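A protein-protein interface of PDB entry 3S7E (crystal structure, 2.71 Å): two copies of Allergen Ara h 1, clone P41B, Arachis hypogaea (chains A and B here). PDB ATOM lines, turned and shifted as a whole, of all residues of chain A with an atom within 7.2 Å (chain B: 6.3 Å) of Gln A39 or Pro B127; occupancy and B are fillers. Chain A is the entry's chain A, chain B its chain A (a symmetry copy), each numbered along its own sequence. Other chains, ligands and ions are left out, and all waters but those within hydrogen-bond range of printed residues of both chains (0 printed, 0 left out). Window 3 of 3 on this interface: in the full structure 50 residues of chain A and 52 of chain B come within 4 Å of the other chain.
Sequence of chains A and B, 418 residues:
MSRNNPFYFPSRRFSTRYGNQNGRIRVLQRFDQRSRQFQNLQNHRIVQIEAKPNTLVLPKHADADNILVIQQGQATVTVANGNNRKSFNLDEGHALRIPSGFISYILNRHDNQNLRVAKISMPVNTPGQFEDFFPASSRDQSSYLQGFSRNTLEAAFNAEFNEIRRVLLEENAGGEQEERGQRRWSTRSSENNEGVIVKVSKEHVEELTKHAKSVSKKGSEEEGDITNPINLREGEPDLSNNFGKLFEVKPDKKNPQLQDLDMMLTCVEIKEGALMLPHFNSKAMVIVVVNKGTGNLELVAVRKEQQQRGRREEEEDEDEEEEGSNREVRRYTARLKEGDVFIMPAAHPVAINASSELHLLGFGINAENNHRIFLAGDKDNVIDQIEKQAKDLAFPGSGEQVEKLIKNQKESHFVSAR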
ATOM      1  N   PHE A  31     -25.472  -2.287 -13.679  1.00  0.00           N
ATOM      2  CA  PHE A  31     -25.656  -1.999 -15.109  1.00  0.00           C
ATOM      3  C   PHE A  31     -26.404  -3.087 -15.859  1.00  0.00           C
ATOM      4  O   PHE A  31     -27.122  -2.792 -16.819  1.00  0.00           O
ATOM      5  CB  PHE A  31     -24.312  -1.792 -15.804  1.00  0.00           C
ATOM      6  CG  PHE A  31     -23.541  -0.622 -15.279  1.00  0.00           C
ATOM      7  CD1 PHE A  31     -24.079   0.655 -15.338  1.00  0.00           C
ATOM      8  CD2 PHE A  31     -22.287  -0.798 -14.710  1.00  0.00           C
ATOM      9  CE1 PHE A  31     -23.372   1.743 -14.848  1.00  0.00           C
ATOM     10  CE2 PHE A  31     -21.575   0.276 -14.220  1.00  0.00           C
ATOM     11  CZ  PHE A  31     -22.117   1.552 -14.284  1.00  0.00           C
ATOM     12  N   ASP A  32     -26.222  -4.336 -15.425  1.00  0.00           N
ATOM     13  CA  ASP A  32     -26.900  -5.486 -16.041  1.00  0.00           C
ATOM     14  C   ASP A  32     -28.307  -5.610 -15.445  1.00  0.00           C
ATOM     15  O   ASP A  32     -28.586  -6.425 -14.555  1.00  0.00           O
ATOM     16  CB  ASP A  32     -26.088  -6.792 -15.927  1.00  0.00           C
ATOM     17  CG  ASP A  32     -26.055  -7.366 -14.513  1.00  0.00           C
ATOM     18  OD1 ASP A  32     -26.795  -8.341 -14.250  1.00  0.00           O
ATOM     19  OD2 ASP A  32     -25.292  -6.852 -13.671  1.00  0.00           O
ATOM     20  N   GLN A  33     -29.171  -4.750 -15.951  1.00  0.00           N
ATOM     21  CA  GLN A  33     -30.570  -4.714 -15.578  1.00  0.00           C
ATOM     22  C   GLN A  33     -31.260  -3.998 -16.736  1.00  0.00           C
ATOM     23  O   GLN A  33     -31.947  -4.618 -17.564  1.00  0.00           O
ATOM     24  CB  GLN A  33     -30.755  -3.937 -14.269  1.00  0.00           C
ATOM     25  N   SER A  35     -30.052  -2.986 -19.455  1.00  0.00           N
ATOM     26  CA  SER A  35     -29.683  -3.556 -20.749  1.00  0.00           C
ATOM     27  C   SER A  35     -28.482  -4.497 -20.664  1.00  0.00           C
ATOM     28  O   SER A  35     -27.586  -4.308 -19.831  1.00  0.00           O
ATOM     29  CB  SER A  35     -29.378  -2.433 -21.749  1.00  0.00           C
ATOM     30  OG  SER A  35     -29.328  -2.920 -23.078  1.00  0.00           O
ATOM     31  N   ARG A  36     -28.478  -5.504 -21.536  1.00  0.00           N
ATOM     32  CA  ARG A  36     -27.304  -6.342 -21.780  1.00  0.00           C
ATOM     33  C   ARG A  36     -26.333  -5.696 -22.790  1.00  0.00           C
ATOM     34  O   ARG A  36     -25.390  -6.347 -23.260  1.00  0.00           O
ATOM     35  CB  ARG A  36     -27.742  -7.717 -22.286  1.00  0.00           C
ATOM     36  N   GLN A  37     -26.562  -4.423 -23.112  1.00  0.00           N
ATOM     37  CA  GLN A  37     -25.702  -3.668 -24.031  1.00  0.00           C
ATOM     38  C   GLN A  37     -24.296  -3.497 -23.482  1.00  0.00           C
ATOM     39  O   GLN A  37     -23.335  -3.331 -24.236  1.00  0.00           O
ATOM     40  CB  GLN A  37     -26.349  -2.335 -24.431  1.00  0.00           C
ATOM     41  CG  GLN A  37     -26.990  -2.376 -25.806  1.00  0.00           C
ATOM     42  CD  GLN A  37     -27.923  -1.210 -26.055  1.00  0.00           C
ATOM     43  OE1 GLN A  37     -28.741  -0.863 -25.202  1.00  0.00           O
ATOM     44  NE2 GLN A  37     -27.810  -0.598 -27.236  1.00  0.00           N
ATOM     45  N   PHE A  38     -24.201  -3.496 -22.161  1.00  0.00           N
ATOM     46  CA  PHE A  38     -22.924  -3.634 -21.457  1.00  0.00           C
ATOM     47  C   PHE A  38     -23.096  -4.607 -20.297  1.00  0.00           C
ATOM     48  O   PHE A  38     -23.103  -4.225 -19.127  1.00  0.00           O
ATOM     49  CB  PHE A  38     -22.379  -2.259 -21.033  1.00  0.00           C
ATOM     50  CG  PHE A  38     -23.440  -1.217 -20.797  1.00  0.00           C
ATOM     51  CD1 PHE A  38     -23.863  -0.394 -21.829  1.00  0.00           C
ATOM     52  CD2 PHE A  38     -24.001  -1.046 -19.545  1.00  0.00           C
ATOM     53  CE1 PHE A  38     -24.838   0.573 -21.611  1.00  0.00           C
ATOM     54  CE2 PHE A  38     -24.975  -0.084 -19.327  1.00  0.00           C
ATOM     55  CZ  PHE A  38     -25.389   0.726 -20.363  1.00  0.00           C
ATOM     56  N   GLN A  39     -23.286  -5.868 -20.656  1.00  0.00           N
ATOM     57  CA  GLN A  39     -23.238  -6.973 -19.703  1.00  0.00           C
ATOM     58  C   GLN A  39     -21.854  -7.095 -19.066  1.00  0.00           C
ATOM     59  O   GLN A  39     -21.726  -7.327 -17.872  1.00  0.00           O
ATOM     60  CB  GLN A  39     -23.564  -8.294 -20.422  1.00  0.00           C
ATOM     61  CG  GLN A  39     -23.569  -9.546 -19.546  1.00  0.00           C
ATOM     62  CD  GLN A  39     -24.630  -9.517 -18.448  1.00  0.00           C
ATOM     63  OE1 GLN A  39     -25.528  -8.670 -18.447  1.00  0.00           O
ATOM     64  NE2 GLN A  39     -24.527 -10.453 -17.507  1.00  0.00           N
ATOM     65  N   ASN A  40     -20.824  -6.902 -19.882  1.00  0.00           N
ATOM     66  CA  ASN A  40     -19.431  -7.054 -19.450  1.00  0.00           C
ATOM     67  C   ASN A  40     -18.945  -5.973 -18.448  1.00  0.00           C
ATOM     68  O   ASN A  40     -17.785  -5.973 -18.045  1.00  0.00           O
ATOM     69  CB  ASN A  40     -18.504  -7.077 -20.675  1.00  0.00           C
ATOM     70  CG  ASN A  40     -18.604  -8.376 -21.475  1.00  0.00           C
ATOM     71  OD1 ASN A  40     -18.618  -9.468 -20.913  1.00  0.00           O
ATOM     72  ND2 ASN A  40     -18.653  -8.255 -22.798  1.00  0.00           N
ATOM     73  N   LEU A  41     -19.831  -5.063 -18.053  1.00  0.00           N
ATOM     74  CA  LEU A  41     -19.541  -4.093 -16.979  1.00  0.00           C
ATOM     75  C   LEU A  41     -20.137  -4.526 -15.624  1.00  0.00           C
ATOM     76  O   LEU A  41     -19.890  -3.892 -14.602  1.00  0.00           O
ATOM     77  CB  LEU A  41     -20.073  -2.692 -17.344  1.00  0.00           C
ATOM     78  CG  LEU A  41     -19.209  -1.769 -18.213  1.00  0.00           C
ATOM     79  CD1 LEU A  41     -19.836  -0.399 -18.388  1.00  0.00           C
ATOM     80  CD2 LEU A  41     -17.830  -1.620 -17.598  1.00  0.00           C
ATOM     81  N   GLN A  42     -20.899  -5.615 -15.620  1.00  0.00           N
ATOM     82  CA  GLN A  42     -21.653  -6.061 -14.438  1.00  0.00           C
ATOM     83  C   GLN A  42     -20.871  -6.199 -13.128  1.00  0.00           C
ATOM     84  O   GLN A  42     -21.473  -6.138 -12.057  1.00  0.00           O
ATOM     85  CB  GLN A  42     -22.372  -7.386 -14.720  1.00  0.00           C
ATOM     86  CG  GLN A  42     -21.470  -8.556 -15.105  1.00  0.00           C
ATOM     87  CD  GLN A  42     -22.175  -9.893 -14.977  1.00  0.00           C
ATOM     88  OE1 GLN A  42     -23.336  -9.959 -14.559  1.00  0.00           O
ATOM     89  NE2 GLN A  42     -21.479 -10.968 -15.330  1.00  0.00           N
ATOM     90  N   ASN A  43     -19.557  -6.392 -13.190  1.00  0.00           N
ATOM     91  CA  ASN A  43     -18.753  -6.450 -11.949  1.00  0.00           C
ATOM     92  C   ASN A  43     -18.304  -5.068 -11.437  1.00  0.00           C
ATOM     93  O   ASN A  43     -17.612  -4.964 -10.425  1.00  0.00           O
ATOM     94  CB  ASN A  43     -17.542  -7.364 -12.107  1.00  0.00           C
ATOM     95  CG  ASN A  43     -17.034  -7.871 -10.779  1.00  0.00           C
ATOM     96  OD1 ASN A  43     -15.972  -7.474 -10.320  1.00  0.00           O
ATOM     97  ND2 ASN A  43     -17.810  -8.729 -10.140  1.00  0.00           N
ATOM     98  N   MET A 285     -13.830   0.388 -22.139  1.00  0.00           N
ATOM     99  CA  MET A 285     -15.252   0.623 -21.886  1.00  0.00           C
ATOM    100  C   MET A 285     -15.297   1.591 -20.740  1.00  0.00           C
ATOM    101  O   MET A 285     -14.961   1.215 -19.633  1.00  0.00           O
ATOM    102  CB  MET A 285     -15.978  -0.658 -21.453  1.00  0.00           C
ATOM    103  CG  MET A 285     -16.537  -1.507 -22.575  1.00  0.00           C
ATOM    104  SD  MET A 285     -17.195  -3.080 -21.956  1.00  0.00           S
ATOM    105  CE  MET A 285     -15.703  -4.001 -21.635  1.00  0.00           C
ATOM    106  N   ARG B  30     -24.327 -17.102 -33.146  1.00  0.00           N
ATOM    107  CA  ARG B  30     -23.754 -17.296 -31.818  1.00  0.00           C
ATOM    108  C   ARG B  30     -23.841 -18.757 -31.353  1.00  0.00           C
ATOM    109  O   ARG B  30     -24.940 -19.294 -31.168  1.00  0.00           O
ATOM    110  CB  ARG B  30     -24.486 -16.401 -30.812  1.00  0.00           C
ATOM    111  CG  ARG B  30     -24.226 -14.921 -31.013  1.00  0.00           C
ATOM    112  CD  ARG B  30     -25.308 -14.019 -30.417  1.00  0.00           C
ATOM    113  NE  ARG B  30     -25.420 -14.164 -28.966  1.00  0.00           N
ATOM    114  CZ  ARG B  30     -25.976 -13.274 -28.145  1.00  0.00           C
ATOM    115  NH1 ARG B  30     -26.020 -13.535 -26.841  1.00  0.00           N
ATOM    116  NH2 ARG B  30     -26.480 -12.128 -28.602  1.00  0.00           N
ATOM    117  N   GLN B  42     -18.817 -18.505 -26.669  1.00  0.00           N
ATOM    118  CA  GLN B  42     -19.788 -17.446 -26.987  1.00  0.00           C
ATOM    119  C   GLN B  42     -19.221 -16.089 -27.412  1.00  0.00           C
ATOM    120  O   GLN B  42     -19.915 -15.329 -28.086  1.00  0.00           O
ATOM    121  CB  GLN B  42     -20.758 -17.228 -25.819  1.00  0.00           C
ATOM    122  CG  GLN B  42     -20.115 -16.819 -24.497  1.00  0.00           C
ATOM    123  CD  GLN B  42     -21.122 -16.239 -23.522  1.00  0.00           C
ATOM    124  OE1 GLN B  42     -22.307 -16.103 -23.842  1.00  0.00           O
ATOM    125  NE2 GLN B  42     -20.658 -15.891 -22.326  1.00  0.00           N
ATOM    126  N   ASN B  43     -17.990 -15.766 -27.026  1.00  0.00           N
ATOM    127  CA  ASN B  43     -17.375 -14.499 -27.480  1.00  0.00           C
ATOM    128  C   ASN B  43     -16.680 -14.605 -28.850  1.00  0.00           C
ATOM    129  O   ASN B  43     -16.107 -13.636 -29.345  1.00  0.00           O
ATOM    130  CB  ASN B  43     -16.400 -13.946 -26.445  1.00  0.00           C
ATOM    131  CG  ASN B  43     -16.185 -12.460 -26.602  1.00  0.00           C
ATOM    132  OD1 ASN B  43     -15.122 -12.020 -27.016  1.00  0.00           O
ATOM    133  ND2 ASN B  43     -17.209 -11.681 -26.301  1.00  0.00           N
ATOM    134  N   HIS B  44     -16.735 -15.784 -29.456  1.00  0.00           N
ATOM    135  CA  HIS B  44     -16.057 -16.026 -30.722  1.00  0.00           C
ATOM    136  C   HIS B  44     -17.042 -16.267 -31.835  1.00  0.00           C
ATOM    137  O   HIS B  44     -17.685 -17.306 -31.915  1.00  0.00           O
ATOM    138  CB  HIS B  44     -15.086 -17.161 -30.556  1.00  0.00           C
ATOM    139  CG  HIS B  44     -14.023 -16.844 -29.569  1.00  0.00           C
ATOM    140  ND1 HIS B  44     -14.196 -17.036 -28.218  1.00  0.00           N
ATOM    141  CD2 HIS B  44     -12.816 -16.251 -29.719  1.00  0.00           C
ATOM    142  CE1 HIS B  44     -13.115 -16.625 -27.579  1.00  0.00           C
ATOM    143  NE2 HIS B  44     -12.261 -16.148 -28.467  1.00  0.00           N
ATOM    144  N   ARG B  45     -17.171 -15.235 -32.663  1.00  0.00           N
ATOM    145  CA  ARG B  45     -18.087 -15.197 -33.798  1.00  0.00           C
ATOM    146  C   ARG B  45     -17.270 -15.321 -35.085  1.00  0.00           C
ATOM    147  O   ARG B  45     -16.188 -14.747 -35.198  1.00  0.00           O
ATOM    148  CB  ARG B  45     -18.869 -13.879 -33.785  1.00  0.00           C
ATOM    149  CG  ARG B  45     -19.844 -13.742 -32.607  1.00  0.00           C
ATOM    150  CD  ARG B  45     -21.029 -14.700 -32.734  1.00  0.00           C
ATOM    151  NE  ARG B  45     -21.570 -14.686 -34.093  1.00  0.00           N
ATOM    152  CZ  ARG B  45     -22.409 -13.771 -34.568  1.00  0.00           C
ATOM    153  NH1 ARG B  45     -22.804 -13.854 -35.830  1.00  0.00           N
ATOM    154  NH2 ARG B  45     -22.850 -12.778 -33.797  1.00  0.00           N
ATOM    155  N   MET B 122     -14.167 -11.010 -31.987  1.00  0.00           N
ATOM    156  CA  MET B 122     -14.143 -11.095 -30.518  1.00  0.00           C
ATOM    157  C   MET B 122     -14.823  -9.821 -29.933  1.00  0.00           C
ATOM    158  O   MET B 122     -14.154  -8.795 -29.782  1.00  0.00           O
ATOM    159  CB  MET B 122     -12.686 -11.137 -30.024  1.00  0.00           C
ATOM    160  CG  MET B 122     -11.946 -12.489 -29.883  1.00  0.00           C
ATOM    161  SD  MET B 122     -11.069 -13.183 -31.314  1.00  0.00           S
ATOM    162  CE  MET B 122     -10.489 -11.767 -32.234  1.00  0.00           C
ATOM    163  N   PRO B 123     -16.144  -9.867 -29.620  1.00  0.00           N
ATOM    164  CA  PRO B 123     -16.886  -8.716 -29.128  1.00  0.00           C
ATOM    165  C   PRO B 123     -16.427  -8.176 -27.783  1.00  0.00           C
ATOM    166  O   PRO B 123     -16.240  -8.929 -26.835  1.00  0.00           O
ATOM    167  CB  PRO B 123     -18.300  -9.256 -29.037  1.00  0.00           C
ATOM    168  CG  PRO B 123     -18.345 -10.205 -30.096  1.00  0.00           C
ATOM    169  CD  PRO B 123     -17.092 -10.945 -29.925  1.00  0.00           C
ATOM    170  N   VAL B 124     -16.266  -6.856 -27.727  1.00  0.00           N
ATOM    171  CA  VAL B 124     -15.750  -6.149 -26.539  1.00  0.00           C
ATOM    172  C   VAL B 124     -16.855  -5.776 -25.571  1.00  0.00           C
ATOM    173  O   VAL B 124     -16.728  -5.942 -24.374  1.00  0.00           O
ATOM    174  CB  VAL B 124     -14.958  -4.845 -26.925  1.00  0.00           C
ATOM    175  CG1 VAL B 124     -14.591  -4.029 -25.685  1.00  0.00           C
ATOM    176  CG2 VAL B 124     -13.683  -5.180 -27.726  1.00  0.00           C
ATOM    177  N   ASN B 125     -17.948  -5.257 -26.085  1.00  0.00           N
ATOM    178  CA  ASN B 125     -18.953  -4.678 -25.204  1.00  0.00           C
ATOM    179  C   ASN B 125     -19.968  -5.696 -24.730  1.00  0.00           C
ATOM    180  O   ASN B 125     -20.204  -5.835 -23.537  1.00  0.00           O
ATOM    181  CB  ASN B 125     -19.660  -3.507 -25.881  1.00  0.00           C
ATOM    182  CG  ASN B 125     -18.697  -2.409 -26.287  1.00  0.00           C
ATOM    183  OD1 ASN B 125     -17.969  -1.872 -25.457  1.00  0.00           O
ATOM    184  ND2 ASN B 125     -18.690  -2.068 -27.562  1.00  0.00           N
ATOM    185  N   THR B 126     -20.552  -6.412 -25.676  1.00  0.00           N
ATOM    186  CA  THR B 126     -21.625  -7.351 -25.378  1.00  0.00           C
ATOM    187  C   THR B 126     -21.108  -8.739 -25.729  1.00  0.00           C
ATOM    188  O   THR B 126     -20.570  -8.934 -26.811  1.00  0.00           O
ATOM    189  CB  THR B 126     -22.949  -7.010 -26.135  1.00  0.00           C
ATOM    190  OG1 THR B 126     -23.390  -5.691 -25.761  1.00  0.00           O
ATOM    191  CG2 THR B 126     -24.053  -8.017 -25.814  1.00  0.00           C
ATOM    192  N   PRO B 127     -21.269  -9.706 -24.809  1.00  0.00           N
ATOM    193  CA  PRO B 127     -20.552 -10.974 -24.886  1.00  0.00           C
ATOM    194  C   PRO B 127     -20.581 -11.646 -26.239  1.00  0.00           C
ATOM    195  O   PRO B 127     -19.540 -12.109 -26.704  1.00  0.00           O
ATOM    196  CB  PRO B 127     -21.268 -11.838 -23.847  1.00  0.00           C
ATOM    197  CG  PRO B 127     -21.704 -10.861 -22.824  1.00  0.00           C
ATOM    198  CD  PRO B 127     -22.115  -9.648 -23.604  1.00  0.00           C
ATOM    199  N   GLY B 128     -21.753 -11.698 -26.857  1.00  0.00           N
ATOM    200  CA  GLY B 128     -21.916 -12.351 -28.153  1.00  0.00           C
ATOM    201  C   GLY B 128     -21.996 -11.432 -29.360  1.00  0.00           C
ATOM    202  O   GLY B 128     -21.966 -11.919 -30.494  1.00  0.00           O
ATOM    203  N   GLN B 129     -22.076 -10.121 -29.133  1.00  0.00           N
ATOM    204  CA  GLN B 129     -22.435  -9.173 -30.202  1.00  0.00           C
ATOM    205  C   GLN B 129     -21.383  -8.114 -30.542  1.00  0.00           C
ATOM    206  O   GLN B 129     -20.750  -7.544 -29.654  1.00  0.00           O
ATOM    207  CB  GLN B 129     -23.744  -8.456 -29.863  1.00  0.00           C
ATOM    208  CG  GLN B 129     -24.879  -9.379 -29.407  1.00  0.00           C
ATOM    209  CD  GLN B 129     -26.237  -8.963 -29.957  1.00  0.00           C
ATOM    210  OE1 GLN B 129     -26.321  -8.259 -30.967  1.00  0.00           O
ATOM    211  NE2 GLN B 129     -27.309  -9.394 -29.295  1.00  0.00           N
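O of Arg A36 is in hydrogen-bond range of OG1 of Thr B126 (3.3 Å).
O of Gln A37 lies within hydrogen-bond range of OG1 of Thr B126, 2.8 Å away.
ND2 of Asn A40 sits at hydrogen-bond distance from O of Val B124.
The side-chain amide nitrogen (ND2) of Asn A40 lies within hydrogen-bond range of the backbone carbonyl oxygen (O) of Asn B125, 3.0 Å away.
The side-chain sulfur of Met A285 lies close to the side-chain amide oxygen of Asn B125 (3.8 Å).
The backbone carbonyl oxygen of Val B124 lies close to the side-chain sulfur of Met A285 (3.8 Å).
Printed residues of chain A within 4 Å of Pro B127: Gln A39 and Asn A40.
Printed residues of chain B within 4 Å of Gln A37: Thr B126 (2.8 Å).
Printed residues of chain B within 4 Å of Asn A40: Val B124, Asn B125, Thr B126 and Pro B127.
Printed residues of chain B within 4 Å of Arg A36: Thr B126 (3.3 Å).
The nearest printed residue of chain A that does not touch Asn B125 is Gln A37 (4.03 Å).
OG of Ser A35 sits at hydrogen-bond distance from OE1 of Gln A37, 3.0 Å away.
The side-chain amide oxygen (OE1) of Gln A42 lies within hydrogen-bond range of the side-chain amide nitrogen (NE2) of Gln A39 (3.2 Å).
O of Pro B127 is in hydrogen-bond range of ND2 of Asn B43, 2.4 Å away.
CB of Gln A39 touches CD of Pro B127, at 3.7 Å.
Thr B126 touches Asn A40.
ND2 of Asn A40 touches N of Pro B127, at 3.6 Å.
Positions printed for both chains: 42 and 43.
Of the 9 pairs that touch across the chains among the printed residues, none has its exchanged pair printed and touching as well.
Hydrophobic or aromatic side chains of chain B within 4 Å of the printed part of chain A: Pro B127.
Of the 13 printed residues of chain A, 5 touch a printed residue of chain B.
Among the printed residues, no Asp or Glu carboxylate lies within 4 Å of a Lys or Arg side-chain nitrogen of the other chain.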
